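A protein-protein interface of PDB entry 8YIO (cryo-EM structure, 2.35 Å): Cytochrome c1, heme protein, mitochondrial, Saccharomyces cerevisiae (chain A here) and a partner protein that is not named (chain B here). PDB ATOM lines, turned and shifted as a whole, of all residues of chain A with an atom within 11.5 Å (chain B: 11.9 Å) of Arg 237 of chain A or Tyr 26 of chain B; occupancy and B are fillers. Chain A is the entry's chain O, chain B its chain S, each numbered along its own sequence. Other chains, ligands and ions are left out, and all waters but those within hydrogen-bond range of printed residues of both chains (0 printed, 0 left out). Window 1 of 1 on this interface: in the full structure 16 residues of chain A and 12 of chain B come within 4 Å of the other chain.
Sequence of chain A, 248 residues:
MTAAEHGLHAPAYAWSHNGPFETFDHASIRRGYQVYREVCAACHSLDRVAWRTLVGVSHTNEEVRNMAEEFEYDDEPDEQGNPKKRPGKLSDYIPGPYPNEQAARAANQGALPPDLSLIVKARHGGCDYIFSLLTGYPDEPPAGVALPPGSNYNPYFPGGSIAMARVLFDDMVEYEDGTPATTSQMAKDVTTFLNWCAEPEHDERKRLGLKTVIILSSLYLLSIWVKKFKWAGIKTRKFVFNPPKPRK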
ATOM      1  N   LYS A 230      25.013  17.145 -14.885  1.00  0.00           N
ATOM      2  CA  LYS A 230      25.602  17.841 -16.019  1.00  0.00           C
ATOM      3  C   LYS A 230      25.546  17.050 -17.320  1.00  0.00           C
ATOM      4  O   LYS A 230      25.923  17.591 -18.362  1.00  0.00           O
ATOM      5  CB  LYS A 230      27.054  18.210 -15.709  1.00  0.00           C
ATOM      6  CG  LYS A 230      27.199  19.302 -14.664  1.00  0.00           C
ATOM      7  CD  LYS A 230      28.586  19.919 -14.691  1.00  0.00           C
ATOM      8  CE  LYS A 230      28.749  20.967 -13.596  1.00  0.00           C
ATOM      9  NZ  LYS A 230      27.707  22.031 -13.641  1.00  0.00           N
ATOM     10  N   TRP A 231      25.084  15.801 -17.294  1.00  0.00           N
ATOM     11  CA  TRP A 231      25.004  14.973 -18.487  1.00  0.00           C
ATOM     12  C   TRP A 231      23.575  14.744 -18.957  1.00  0.00           C
ATOM     13  O   TRP A 231      23.377  14.072 -19.970  1.00  0.00           O
ATOM     14  CB  TRP A 231      25.682  13.616 -18.242  1.00  0.00           C
ATOM     15  CG  TRP A 231      27.126  13.566 -18.649  1.00  0.00           C
ATOM     16  CD1 TRP A 231      28.188  14.056 -17.954  1.00  0.00           C
ATOM     17  CD2 TRP A 231      27.662  12.996 -19.849  1.00  0.00           C
ATOM     18  NE1 TRP A 231      29.350  13.829 -18.641  1.00  0.00           N
ATOM     19  CE2 TRP A 231      29.056  13.180 -19.808  1.00  0.00           C
ATOM     20  CE3 TRP A 231      27.098  12.349 -20.953  1.00  0.00           C
ATOM     21  CZ2 TRP A 231      29.897  12.741 -20.829  1.00  0.00           C
ATOM     22  CZ3 TRP A 231      27.932  11.915 -21.963  1.00  0.00           C
ATOM     23  CH2 TRP A 231      29.316  12.112 -21.896  1.00  0.00           C
ATOM     24  N   ALA A 232      22.578  15.295 -18.260  1.00  0.00           N
ATOM     25  CA  ALA A 232      21.185  14.954 -18.525  1.00  0.00           C
ATOM     26  C   ALA A 232      20.663  15.538 -19.832  1.00  0.00           C
ATOM     27  O   ALA A 232      19.712  14.992 -20.396  1.00  0.00           O
ATOM     28  CB  ALA A 232      20.304  15.411 -17.362  1.00  0.00           C
ATOM     29  N   GLY A 233      21.259  16.624 -20.328  1.00  0.00           N
ATOM     30  CA  GLY A 233      20.844  17.157 -21.615  1.00  0.00           C
ATOM     31  C   GLY A 233      21.270  16.286 -22.783  1.00  0.00           C
ATOM     32  O   GLY A 233      20.553  16.179 -23.779  1.00  0.00           O
ATOM     33  N   ILE A 234      22.440  15.655 -22.676  1.00  0.00           N
ATOM     34  CA  ILE A 234      22.923  14.768 -23.729  1.00  0.00           C
ATOM     35  C   ILE A 234      22.159  13.446 -23.713  1.00  0.00           C
ATOM     36  O   ILE A 234      21.819  12.897 -24.768  1.00  0.00           O
ATOM     37  CB  ILE A 234      24.444  14.561 -23.575  1.00  0.00           C
ATOM     38  CG1 ILE A 234      25.182  15.897 -23.694  1.00  0.00           C
ATOM     39  CG2 ILE A 234      24.987  13.565 -24.588  1.00  0.00           C
ATOM     40  CD1 ILE A 234      25.180  16.483 -25.084  1.00  0.00           C
ATOM     41  N   LYS A 235      21.843  12.934 -22.521  1.00  0.00           N
ATOM     42  CA  LYS A 235      21.256  11.604 -22.394  1.00  0.00           C
ATOM     43  C   LYS A 235      19.803  11.535 -22.855  1.00  0.00           C
ATOM     44  O   LYS A 235      19.320  10.440 -23.151  1.00  0.00           O
ATOM     45  CB  LYS A 235      21.350  11.122 -20.945  1.00  0.00           C
ATOM     46  CG  LYS A 235      22.763  10.870 -20.464  1.00  0.00           C
ATOM     47  CD  LYS A 235      23.114   9.395 -20.453  1.00  0.00           C
ATOM     48  CE  LYS A 235      24.592   9.197 -20.154  1.00  0.00           C
ATOM     49  NZ  LYS A 235      24.909   7.803 -19.753  1.00  0.00           N
ATOM     50  N   THR A 236      19.094  12.662 -22.930  1.00  0.00           N
ATOM     51  CA  THR A 236      17.696  12.665 -23.350  1.00  0.00           C
ATOM     52  C   THR A 236      17.498  13.319 -24.713  1.00  0.00           C
ATOM     53  O   THR A 236      16.373  13.666 -25.074  1.00  0.00           O
ATOM     54  CB  THR A 236      16.823  13.346 -22.293  1.00  0.00           C
ATOM     55  OG1 THR A 236      17.432  14.571 -21.877  1.00  0.00           O
ATOM     56  CG2 THR A 236      16.662  12.446 -21.086  1.00  0.00           C
ATOM     57  N   ARG A 237      18.572  13.466 -25.482  1.00  0.00           N
ATOM     58  CA  ARG A 237      18.524  14.076 -26.805  1.00  0.00           C
ATOM     59  C   ARG A 237      17.830  13.158 -27.815  1.00  0.00           C
ATOM     60  O   ARG A 237      17.986  11.937 -27.773  1.00  0.00           O
ATOM     61  CB  ARG A 237      19.953  14.391 -27.239  1.00  0.00           C
ATOM     62  CG  ARG A 237      20.127  15.200 -28.486  1.00  0.00           C
ATOM     63  CD  ARG A 237      21.593  15.553 -28.651  1.00  0.00           C
ATOM     64  NE  ARG A 237      22.458  14.403 -28.413  1.00  0.00           N
ATOM     65  CZ  ARG A 237      23.761  14.375 -28.674  1.00  0.00           C
ATOM     66  NH1 ARG A 237      24.464  13.280 -28.428  1.00  0.00           N
ATOM     67  NH2 ARG A 237      24.361  15.438 -29.182  1.00  0.00           N
ATOM     68  N   LYS A 238      17.053  13.752 -28.726  1.00  0.00           N
ATOM     69  CA  LYS A 238      16.269  13.010 -29.709  1.00  0.00           C
ATOM     70  C   LYS A 238      16.585  13.469 -31.129  1.00  0.00           C
ATOM     71  O   LYS A 238      16.856  14.645 -31.365  1.00  0.00           O
ATOM     72  CB  LYS A 238      14.766  13.163 -29.442  1.00  0.00           C
ATOM     73  CG  LYS A 238      14.349  12.716 -28.060  1.00  0.00           C
ATOM     74  CD  LYS A 238      12.862  12.788 -27.864  1.00  0.00           C
ATOM     75  CE  LYS A 238      12.504  12.585 -26.408  1.00  0.00           C
ATOM     76  NZ  LYS A 238      13.105  11.339 -25.858  1.00  0.00           N
ATOM     77  N   PHE A 239      16.530  12.529 -32.079  1.00  0.00           N
ATOM     78  CA  PHE A 239      16.855  12.781 -33.482  1.00  0.00           C
ATOM     79  C   PHE A 239      15.710  12.344 -34.387  1.00  0.00           C
ATOM     80  O   PHE A 239      15.028  11.357 -34.105  1.00  0.00           O
ATOM     81  CB  PHE A 239      18.133  12.045 -33.907  1.00  0.00           C
ATOM     82  CG  PHE A 239      19.390  12.596 -33.300  1.00  0.00           C
ATOM     83  CD1 PHE A 239      20.090  13.612 -33.925  1.00  0.00           C
ATOM     84  CD2 PHE A 239      19.884  12.082 -32.110  1.00  0.00           C
ATOM     85  CE1 PHE A 239      21.254  14.115 -33.372  1.00  0.00           C
ATOM     86  CE2 PHE A 239      21.047  12.582 -31.552  1.00  0.00           C
ATOM     87  CZ  PHE A 239      21.731  13.600 -32.184  1.00  0.00           C
ATOM     88  N   VAL A 240      15.510  13.080 -35.480  1.00  0.00           N
ATOM     89  CA  VAL A 240      14.455  12.814 -36.457  1.00  0.00           C
ATOM     90  C   VAL A 240      15.044  12.990 -37.855  1.00  0.00           C
ATOM     91  O   VAL A 240      15.746  13.971 -38.118  1.00  0.00           O
ATOM     92  CB  VAL A 240      13.236  13.748 -36.231  1.00  0.00           C
ATOM     93  CG1 VAL A 240      12.340  13.830 -37.451  1.00  0.00           C
ATOM     94  CG2 VAL A 240      12.415  13.298 -35.036  1.00  0.00           C
ATOM     95  N   PHE A 241      14.774  12.038 -38.749  1.00  0.00           N
ATOM     96  CA  PHE A 241      15.273  12.076 -40.119  1.00  0.00           C
ATOM     97  C   PHE A 241      14.132  12.269 -41.107  1.00  0.00           C
ATOM     98  O   PHE A 241      13.166  11.501 -41.105  1.00  0.00           O
ATOM     99  CB  PHE A 241      16.034  10.795 -40.459  1.00  0.00           C
ATOM    100  CG  PHE A 241      16.674  10.809 -41.819  1.00  0.00           C
ATOM    101  CD1 PHE A 241      17.488  11.861 -42.207  1.00  0.00           C
ATOM    102  CD2 PHE A 241      16.471   9.763 -42.704  1.00  0.00           C
ATOM    103  CE1 PHE A 241      18.082  11.874 -43.457  1.00  0.00           C
ATOM    104  CE2 PHE A 241      17.063   9.769 -43.956  1.00  0.00           C
ATOM    105  CZ  PHE A 241      17.870  10.824 -44.332  1.00  0.00           C
ATOM    106  N   ASN A 242      14.253  13.286 -41.953  1.00  0.00           N
ATOM    107  CA  ASN A 242      13.370  13.477 -43.096  1.00  0.00           C
ATOM    108  C   ASN A 242      14.220  13.447 -44.359  1.00  0.00           C
ATOM    109  O   ASN A 242      15.133  14.278 -44.494  1.00  0.00           O
ATOM    110  CB  ASN A 242      12.603  14.799 -42.998  1.00  0.00           C
ATOM    111  CG  ASN A 242      11.554  14.786 -41.907  1.00  0.00           C
ATOM    112  OD1 ASN A 242      11.783  15.278 -40.805  1.00  0.00           O
ATOM    113  ND2 ASN A 242      10.397  14.223 -42.210  1.00  0.00           N
ATOM    114  N   TRP B  12      36.748  21.891 -35.044  1.00  0.00           N
ATOM    115  CA  TRP B  12      35.365  22.372 -35.033  1.00  0.00           C
ATOM    116  C   TRP B  12      35.077  23.250 -36.249  1.00  0.00           C
ATOM    117  O   TRP B  12      35.723  24.282 -36.451  1.00  0.00           O
ATOM    118  CB  TRP B  12      35.085  23.152 -33.747  1.00  0.00           C
ATOM    119  CG  TRP B  12      35.245  22.369 -32.471  1.00  0.00           C
ATOM    120  CD1 TRP B  12      36.277  22.452 -31.588  1.00  0.00           C
ATOM    121  CD2 TRP B  12      34.333  21.404 -31.930  1.00  0.00           C
ATOM    122  NE1 TRP B  12      36.074  21.595 -30.539  1.00  0.00           N
ATOM    123  CE2 TRP B  12      34.887  20.939 -30.723  1.00  0.00           C
ATOM    124  CE3 TRP B  12      33.106  20.883 -32.353  1.00  0.00           C
ATOM    125  CZ2 TRP B  12      34.257  19.979 -29.932  1.00  0.00           C
ATOM    126  CZ3 TRP B  12      32.484  19.932 -31.569  1.00  0.00           C
ATOM    127  CH2 TRP B  12      33.059  19.490 -30.371  1.00  0.00           C
ATOM    128  N   GLN B  20      25.911  16.406 -44.041  1.00  0.00           N
ATOM    129  CA  GLN B  20      24.667  16.070 -43.369  1.00  0.00           C
ATOM    130  C   GLN B  20      23.538  16.950 -43.883  1.00  0.00           C
ATOM    131  O   GLN B  20      23.709  18.160 -44.054  1.00  0.00           O
ATOM    132  CB  GLN B  20      24.803  16.231 -41.854  1.00  0.00           C
ATOM    133  CG  GLN B  20      25.891  15.385 -41.236  1.00  0.00           C
ATOM    134  CD  GLN B  20      25.904  15.472 -39.727  1.00  0.00           C
ATOM    135  OE1 GLN B  20      24.886  15.764 -39.105  1.00  0.00           O
ATOM    136  NE2 GLN B  20      27.060  15.217 -39.129  1.00  0.00           N
ATOM    137  N   GLY B  22      19.024  16.898 -43.534  1.00  0.00           N
ATOM    138  CA  GLY B  22      17.747  16.292 -43.227  1.00  0.00           C
ATOM    139  C   GLY B  22      17.557  15.803 -41.807  1.00  0.00           C
ATOM    140  O   GLY B  22      16.511  15.219 -41.515  1.00  0.00           O
ATOM    141  N   ILE B  23      18.518  16.028 -40.917  1.00  0.00           N
ATOM    142  CA  ILE B  23      18.471  15.530 -39.546  1.00  0.00           C
ATOM    143  C   ILE B  23      18.225  16.700 -38.603  1.00  0.00           C
ATOM    144  O   ILE B  23      18.949  17.702 -38.644  1.00  0.00           O
ATOM    145  CB  ILE B  23      19.769  14.788 -39.180  1.00  0.00           C
ATOM    146  CG1 ILE B  23      20.026  13.649 -40.167  1.00  0.00           C
ATOM    147  CG2 ILE B  23      19.714  14.266 -37.755  1.00  0.00           C
ATOM    148  CD1 ILE B  23      21.319  12.920 -39.943  1.00  0.00           C
ATOM    149  N   THR B  24      17.205  16.575 -37.758  1.00  0.00           N
ATOM    150  CA  THR B  24      16.873  17.560 -36.737  1.00  0.00           C
ATOM    151  C   THR B  24      17.090  16.955 -35.354  1.00  0.00           C
ATOM    152  O   THR B  24      16.796  15.778 -35.134  1.00  0.00           O
ATOM    153  CB  THR B  24      15.420  18.031 -36.890  1.00  0.00           C
ATOM    154  OG1 THR B  24      15.142  18.267 -38.274  1.00  0.00           O
ATOM    155  CG2 THR B  24      15.167  19.316 -36.123  1.00  0.00           C
ATOM    156  N   SER B  25      17.612  17.753 -34.423  1.00  0.00           N
ATOM    157  CA  SER B  25      17.830  17.307 -33.052  1.00  0.00           C
ATOM    158  C   SER B  25      17.167  18.255 -32.058  1.00  0.00           C
ATOM    159  O   SER B  25      17.018  19.450 -32.319  1.00  0.00           O
ATOM    160  CB  SER B  25      19.327  17.173 -32.735  1.00  0.00           C
ATOM    161  OG  SER B  25      20.037  18.338 -33.085  1.00  0.00           O
ATOM    162  N   TYR B  26      16.775  17.702 -30.910  1.00  0.00           N
ATOM    163  CA  TYR B  26      16.065  18.419 -29.857  1.00  0.00           C
ATOM    164  C   TYR B  26      16.681  18.088 -28.504  1.00  0.00           C
ATOM    165  O   TYR B  26      17.118  16.957 -28.279  1.00  0.00           O
ATOM    166  CB  TYR B  26      14.571  18.057 -29.832  1.00  0.00           C
ATOM    167  CG  TYR B  26      13.827  18.240 -31.138  1.00  0.00           C
ATOM    168  CD1 TYR B  26      13.746  17.206 -32.064  1.00  0.00           C
ATOM    169  CD2 TYR B  26      13.187  19.438 -31.434  1.00  0.00           C
ATOM    170  CE1 TYR B  26      13.063  17.364 -33.250  1.00  0.00           C
ATOM    171  CE2 TYR B  26      12.499  19.605 -32.617  1.00  0.00           C
ATOM    172  CZ  TYR B  26      12.439  18.563 -33.522  1.00  0.00           C
ATOM    173  OH  TYR B  26      11.761  18.719 -34.704  1.00  0.00           O
ATOM    174  N   ALA B  27      16.699  19.065 -27.598  1.00  0.00           N
ATOM    175  CA  ALA B  27      17.236  18.865 -26.258  1.00  0.00           C
ATOM    176  C   ALA B  27      16.566  19.826 -25.284  1.00  0.00           C
ATOM    177  O   ALA B  27      16.075  20.885 -25.670  1.00  0.00           O
ATOM    178  CB  ALA B  27      18.758  19.047 -26.227  1.00  0.00           C
ATOM    179  N   VAL B  28      16.557  19.438 -24.006  1.00  0.00           N
ATOM    180  CA  VAL B  28      15.968  20.213 -22.918  1.00  0.00           C
ATOM    181  C   VAL B  28      17.065  20.508 -21.896  1.00  0.00           C
ATOM    182  O   VAL B  28      17.975  19.694 -21.708  1.00  0.00           O
ATOM    183  CB  VAL B  28      14.771  19.456 -22.283  1.00  0.00           C
ATOM    184  CG1 VAL B  28      14.101  20.237 -21.159  1.00  0.00           C
ATOM    185  CG2 VAL B  28      13.726  19.149 -23.331  1.00  0.00           C
ATOM    186  N   SER B  29      17.001  21.693 -21.278  1.00  0.00           N
ATOM    187  CA  SER B  29      17.976  22.120 -20.280  1.00  0.00           C
ATOM    188  C   SER B  29      17.990  21.182 -19.072  1.00  0.00           C
ATOM    189  O   SER B  29      16.932  20.715 -18.636  1.00  0.00           O
ATOM    190  CB  SER B  29      17.656  23.540 -19.809  1.00  0.00           C
ATOM    191  OG  SER B  29      18.534  23.953 -18.781  1.00  0.00           O
ATOM    192  N   PRO B  30      19.167  20.887 -18.513  1.00  0.00           N
ATOM    193  CA  PRO B  30      19.225  20.079 -17.282  1.00  0.00           C
ATOM    194  C   PRO B  30      18.617  20.752 -16.063  1.00  0.00           C
ATOM    195  O   PRO B  30      18.238  20.050 -15.119  1.00  0.00           O
ATOM    196  CB  PRO B  30      20.729  19.849 -17.087  1.00  0.00           C
ATOM    197  CG  PRO B  30      21.322  20.050 -18.431  1.00  0.00           C
ATOM    198  CD  PRO B  30      20.501  21.101 -19.093  1.00  0.00           C
ATOM    199  N   GLN B  33      14.832  19.552 -15.597  1.00  0.00           N
ATOM    200  CA  GLN B  33      14.564  18.123 -15.566  1.00  0.00           C
ATOM    201  C   GLN B  33      14.500  17.620 -14.129  1.00  0.00           C
ATOM    202  O   GLN B  33      14.916  18.300 -13.188  1.00  0.00           O
ATOM    203  CB  GLN B  33      15.624  17.348 -16.356  1.00  0.00           C
ATOM    204  CG  GLN B  33      15.631  17.667 -17.841  1.00  0.00           C
ATOM    205  CD  GLN B  33      16.554  16.768 -18.638  1.00  0.00           C
ATOM    206  OE1 GLN B  33      16.600  15.562 -18.419  1.00  0.00           O
ATOM    207  NE2 GLN B  33      17.294  17.353 -19.568  1.00  0.00           N
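Of the 13 printed residues of chain A, 9 touch a printed residue of chain B.
Hydrophobic or aromatic side chains of chain B that line the printed part of chain A: Ile 23 and Pro 30.
The backbone carbonyl oxygen (O) of Val 28 of chain B is in hydrogen-bond range of the side-chain amide nitrogen (NE2) of Gln 33 of chain B, at 3.2 Å.
The backbone carbonyl oxygen of Ala 232 of chain A lies within hydrogen-bond range of the side-chain hydroxyl of Thr 236 of chain A (2.8 Å).
Gly 233 of chain A touches two residues of chain B.
Thr 236 of chain A touches just one residue of chain B: Gln 33.
Of chain B, only Tyr 26 comes within 4 Å of Arg 237 of chain A.
Lys 238 of chain A touches just these residues of chain B: Thr 24 (3.9 Å), Ser 25 (3.3 Å) and Tyr 26 (3.1 Å).
Phe 239 of chain A touches three residues of chain B.
Of chain B, only Gly 22, Ile 23 and Thr 24 come within 4 Å of Val 240 of chain A.
Ser 25 of chain B touches just these residues of chain A: Lys 238 (3.3 Å) and Phe 239 (3.7 Å).
Tyr 26 of chain B touches just these residues of chain A: Arg 237 (3.5 Å) and Lys 238 (3.1 Å).
Ala 27 of chain B touches none of the printed residues of chain A.
Of the printed residues of chain A, Pro 30 of chain B touches Gly 233 (3.9 Å).
Printed residues of chain A within 4 Å of Gln 33 of chain B: Ala 232 (3.5 Å) and Thr 236 (3.6 Å).
The nearest printed residue of chain A that does not touch Gln 33 of chain B is Gly 233 of chain A (4.1 Å).
N of Asn 242 of chain A lies within hydrogen-bond range of O of Gly 22 of chain B, at 3.0 Å.
O of Val 240 of chain A lies within hydrogen-bond range of N of Thr 24 of chain B, at 3.0 Å.
NE2 of Gln 33 of chain B sits at hydrogen-bond distance from O of Ala 232 of chain A, at 3.5 Å.
O of Lys 238 of chain A lies within hydrogen-bond range of N of Tyr 26 of chain B.
Among the printed residues, pairs that only touch across the chains: Gly 233 of chain A with Val 28 of chain B, Gly 233 of chain A with Pro 30 of chain B, Thr 236 of chain A with Gln 33 of chain B, Arg 237 of chain A with Tyr 26 of chain B, Lys 238 of chain A with Thr 24 of chain B, Lys 238 of chain A with Ser 25 of chain B, Phe 239 of chain A with Ile 23 of chain B, Phe 239 of chain A with Thr 24 of chain B, Phe 239 of chain A with Ser 25 of chain B, Val 240 of chain A with Gly 22 of chain B, Val 240 of chain A with Ile 23 of chain B, Phe 241 of chain A with Gly 22 of chain B and Phe 241 of chain A with Ile 23 of chain B.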
